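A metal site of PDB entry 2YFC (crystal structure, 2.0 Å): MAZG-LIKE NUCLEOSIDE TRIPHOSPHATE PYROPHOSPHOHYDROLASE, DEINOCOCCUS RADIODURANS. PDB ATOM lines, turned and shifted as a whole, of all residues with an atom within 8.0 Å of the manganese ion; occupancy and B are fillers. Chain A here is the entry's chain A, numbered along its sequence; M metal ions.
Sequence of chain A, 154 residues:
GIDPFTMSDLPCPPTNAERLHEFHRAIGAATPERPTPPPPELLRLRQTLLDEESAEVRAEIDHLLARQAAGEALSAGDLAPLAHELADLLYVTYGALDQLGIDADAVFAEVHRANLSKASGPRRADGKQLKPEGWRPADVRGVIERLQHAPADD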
ATOM      1  N   LEU A  49      -0.112 -16.699  14.964  1.00  0.00           N
ATOM      2  CA  LEU A  49       0.358 -16.428  13.611  1.00  0.00           C
ATOM      3  C   LEU A  49       1.438 -15.347  13.567  1.00  0.00           C
ATOM      4  O   LEU A  49       2.348 -15.398  12.739  1.00  0.00           O
ATOM      5  CB  LEU A  49      -0.812 -16.023  12.715  1.00  0.00           C
ATOM      6  CG  LEU A  49      -1.915 -17.076  12.548  1.00  0.00           C
ATOM      7  CD1 LEU A  49      -3.164 -16.448  11.963  1.00  0.00           C
ATOM      8  CD2 LEU A  49      -1.428 -18.230  11.677  1.00  0.00           C
ATOM      9  N   GLU A  52       4.651 -17.067  14.747  1.00  0.00           N
ATOM     10  CA  GLU A  52       5.203 -17.946  13.727  1.00  0.00           C
ATOM     11  C   GLU A  52       5.998 -17.174  12.667  1.00  0.00           C
ATOM     12  O   GLU A  52       7.134 -17.506  12.365  1.00  0.00           O
ATOM     13  CB  GLU A  52       4.109 -18.777  13.069  1.00  0.00           C
ATOM     14  CG  GLU A  52       3.584 -19.903  13.973  1.00  0.00           C
ATOM     15  CD  GLU A  52       2.478 -20.727  13.319  1.00  0.00           C
ATOM     16  OE1 GLU A  52       1.990 -20.330  12.238  1.00  0.00           O
ATOM     17  OE2 GLU A  52       2.091 -21.769  13.889  1.00  0.00           O
ATOM     18  N   GLU A  53       5.386 -16.126  12.111  1.00  0.00           N
ATOM     19  CA  GLU A  53       6.043 -15.354  11.072  1.00  0.00           C
ATOM     20  C   GLU A  53       7.196 -14.486  11.616  1.00  0.00           C
ATOM     21  O   GLU A  53       8.204 -14.325  10.935  1.00  0.00           O
ATOM     22  CB  GLU A  53       5.034 -14.505  10.295  1.00  0.00           C
ATOM     23  CG  GLU A  53       3.863 -15.286   9.725  1.00  0.00           C
ATOM     24  CD  GLU A  53       4.284 -16.335   8.684  1.00  0.00           C
ATOM     25  OE1 GLU A  53       5.440 -16.270   8.219  1.00  0.00           O
ATOM     26  OE2 GLU A  53       3.474 -17.198   8.331  1.00  0.00           O
ATOM     27  N   SER A  54       7.054 -13.938  12.821  1.00  0.00           N
ATOM     28  CA  SER A  54       8.145 -13.164  13.418  1.00  0.00           C
ATOM     29  C   SER A  54       9.387 -14.034  13.602  1.00  0.00           C
ATOM     30  O   SER A  54      10.527 -13.579  13.374  1.00  0.00           O
ATOM     31  CB  SER A  54       7.737 -12.571  14.765  1.00  0.00           C
ATOM     32  OG  SER A  54       6.770 -11.556  14.613  1.00  0.00           O
ATOM     33  N   ALA A  55       9.168 -15.276  14.009  1.00  0.00           N
ATOM     34  CA  ALA A  55      10.263 -16.222  14.241  1.00  0.00           C
ATOM     35  C   ALA A  55      10.983 -16.565  12.932  1.00  0.00           C
ATOM     36  O   ALA A  55      12.208 -16.719  12.909  1.00  0.00           O
ATOM     37  CB  ALA A  55       9.747 -17.481  14.947  1.00  0.00           C
ATOM     38  N   GLU A  56      10.225 -16.658  11.845  1.00  0.00           N
ATOM     39  CA  GLU A  56      10.846 -16.930  10.552  1.00  0.00           C
ATOM     40  C   GLU A  56      11.680 -15.726  10.065  1.00  0.00           C
ATOM     41  O   GLU A  56      12.804 -15.910   9.580  1.00  0.00           O
ATOM     42  CB  GLU A  56       9.790 -17.339   9.523  1.00  0.00           C
ATOM     43  CG  GLU A  56       9.200 -18.708   9.860  1.00  0.00           C
ATOM     44  CD  GLU A  56       8.119 -19.159   8.902  1.00  0.00           C
ATOM     45  OE1 GLU A  56       7.447 -18.301   8.291  1.00  0.00           O
ATOM     46  OE2 GLU A  56       7.930 -20.378   8.768  1.00  0.00           O
ATOM     47  N   VAL A  57      11.143 -14.522  10.245  1.00  0.00           N
ATOM     48  CA  VAL A  57      11.918 -13.298   9.947  1.00  0.00           C
ATOM     49  C   VAL A  57      13.216 -13.232  10.770  1.00  0.00           C
ATOM     50  O   VAL A  57      14.321 -13.040  10.216  1.00  0.00           O
ATOM     51  CB  VAL A  57      11.070 -12.034  10.213  1.00  0.00           C
ATOM     52  CG1 VAL A  57      11.976 -10.785  10.224  1.00  0.00           C
ATOM     53  CG2 VAL A  57       9.939 -11.915   9.169  1.00  0.00           C
ATOM     54  N   PRO A  81      14.637 -14.631   0.446  1.00  0.00           N
ATOM     55  CA  PRO A  81      13.892 -15.292   1.513  1.00  0.00           C
ATOM     56  C   PRO A  81      13.474 -14.315   2.633  1.00  0.00           C
ATOM     57  O   PRO A  81      12.382 -14.441   3.162  1.00  0.00           O
ATOM     58  CB  PRO A  81      14.886 -16.337   2.037  1.00  0.00           C
ATOM     59  CG  PRO A  81      15.799 -16.597   0.850  1.00  0.00           C
ATOM     60  CD  PRO A  81      15.958 -15.231   0.237  1.00  0.00           C
ATOM     61  N   HIS A  84      10.464 -12.293   1.485  1.00  0.00           N
ATOM     62  CA  HIS A  84       9.297 -13.171   1.579  1.00  0.00           C
ATOM     63  C   HIS A  84       8.738 -13.256   3.005  1.00  0.00           C
ATOM     64  O   HIS A  84       7.526 -13.105   3.220  1.00  0.00           O
ATOM     65  CB  HIS A  84       9.672 -14.569   1.083  1.00  0.00           C
ATOM     66  CG  HIS A  84       8.491 -15.451   0.825  1.00  0.00           C
ATOM     67  ND1 HIS A  84       8.562 -16.555  -0.003  1.00  0.00           N
ATOM     68  CD2 HIS A  84       7.220 -15.393   1.269  1.00  0.00           C
ATOM     69  CE1 HIS A  84       7.372 -17.137  -0.050  1.00  0.00           C
ATOM     70  NE2 HIS A  84       6.543 -16.455   0.723  1.00  0.00           N
ATOM     71  N   GLU A  85       9.603 -13.524   3.974  1.00  0.00           N
ATOM     72  CA  GLU A  85       9.188 -13.621   5.367  1.00  0.00           C
ATOM     73  C   GLU A  85       8.645 -12.278   5.889  1.00  0.00           C
ATOM     74  O   GLU A  85       7.652 -12.248   6.614  1.00  0.00           O
ATOM     75  CB  GLU A  85      10.325 -14.140   6.259  1.00  0.00           C
ATOM     76  CG  GLU A  85      10.804 -15.537   5.888  1.00  0.00           C
ATOM     77  CD  GLU A  85       9.674 -16.560   5.887  1.00  0.00           C
ATOM     78  OE1 GLU A  85       8.591 -16.261   6.422  1.00  0.00           O
ATOM     79  OE2 GLU A  85       9.864 -17.679   5.355  1.00  0.00           O
ATOM     80  N   LEU A  86       9.283 -11.171   5.514  1.00  0.00           N
ATOM     81  CA  LEU A  86       8.747  -9.847   5.864  1.00  0.00           C
ATOM     82  C   LEU A  86       7.325  -9.628   5.315  1.00  0.00           C
ATOM     83  O   LEU A  86       6.442  -9.126   6.013  1.00  0.00           O
ATOM     84  CB  LEU A  86       9.703  -8.717   5.411  1.00  0.00           C
ATOM     85  CG  LEU A  86      11.003  -8.585   6.228  1.00  0.00           C
ATOM     86  CD1 LEU A  86      12.068  -7.725   5.503  1.00  0.00           C
ATOM     87  CD2 LEU A  86      10.705  -8.054   7.648  1.00  0.00           C
ATOM     88  N   ALA A  87       7.113 -10.026   4.069  1.00  0.00           N
ATOM     89  CA  ALA A  87       5.778  -9.931   3.485  1.00  0.00           C
ATOM     90  C   ALA A  87       4.742 -10.867   4.151  1.00  0.00           C
ATOM     91  O   ALA A  87       3.589 -10.474   4.349  1.00  0.00           O
ATOM     92  CB  ALA A  87       5.842 -10.173   1.966  1.00  0.00           C
ATOM     93  N   ASP A  88       5.153 -12.091   4.519  1.00  0.00           N
ATOM     94  CA  ASP A  88       4.303 -12.975   5.337  1.00  0.00           C
ATOM     95  C   ASP A  88       3.921 -12.289   6.651  1.00  0.00           C
ATOM     96  O   ASP A  88       2.783 -12.392   7.110  1.00  0.00           O
ATOM     97  CB  ASP A  88       5.036 -14.275   5.681  1.00  0.00           C
ATOM     98  CG  ASP A  88       4.973 -15.310   4.578  1.00  0.00           C
ATOM     99  OD1 ASP A  88       4.214 -15.132   3.596  1.00  0.00           O
ATOM    100  OD2 ASP A  88       5.698 -16.322   4.712  1.00  0.00           O
ATOM    101  N   LEU A  89       4.885 -11.616   7.295  1.00  0.00           N
ATOM    102  CA  LEU A  89       4.597 -10.902   8.540  1.00  0.00           C
ATOM    103  C   LEU A  89       3.589  -9.761   8.332  1.00  0.00           C
ATOM    104  O   LEU A  89       2.674  -9.572   9.139  1.00  0.00           O
ATOM    105  CB  LEU A  89       5.891 -10.385   9.191  1.00  0.00           C
ATOM    106  CG  LEU A  89       5.755  -9.664  10.541  1.00  0.00           C
ATOM    107  CD1 LEU A  89       5.038 -10.536  11.598  1.00  0.00           C
ATOM    108  CD2 LEU A  89       7.120  -9.204  11.074  1.00  0.00           C
ATOM    109  N   VAL A  92       0.047 -11.388   8.120  1.00  0.00           N
ATOM    110  CA  VAL A  92      -0.621 -11.798   9.355  1.00  0.00           C
ATOM    111  C   VAL A  92      -0.928 -10.632  10.287  1.00  0.00           C
ATOM    112  O   VAL A  92      -1.827 -10.708  11.114  1.00  0.00           O
ATOM    113  CB  VAL A  92       0.151 -12.874  10.102  1.00  0.00           C
ATOM    114  CG1 VAL A  92       0.290 -14.132   9.237  1.00  0.00           C
ATOM    115  CG2 VAL A  92       1.521 -12.340  10.549  1.00  0.00           C
HETATM  116 MN    MN M   1       6.554 -17.368   6.506  1.00  0.00          MN
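Along chain A the residues within 4 Å of the manganese ion span positions 53 to 88. The nearest printed residue that does not touch the manganese ion is His 84 (5.5 Å).
The manganese ion is bound by the side-chain carboxylate of Glu 56 (2.2 Å), the side-chain carboxylate of Asp 88 (2.2 Å), the side-chain carboxylate of Glu 85 (2.3 Å) and the side-chain carboxylate of Glu 53 (2.3 Å).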
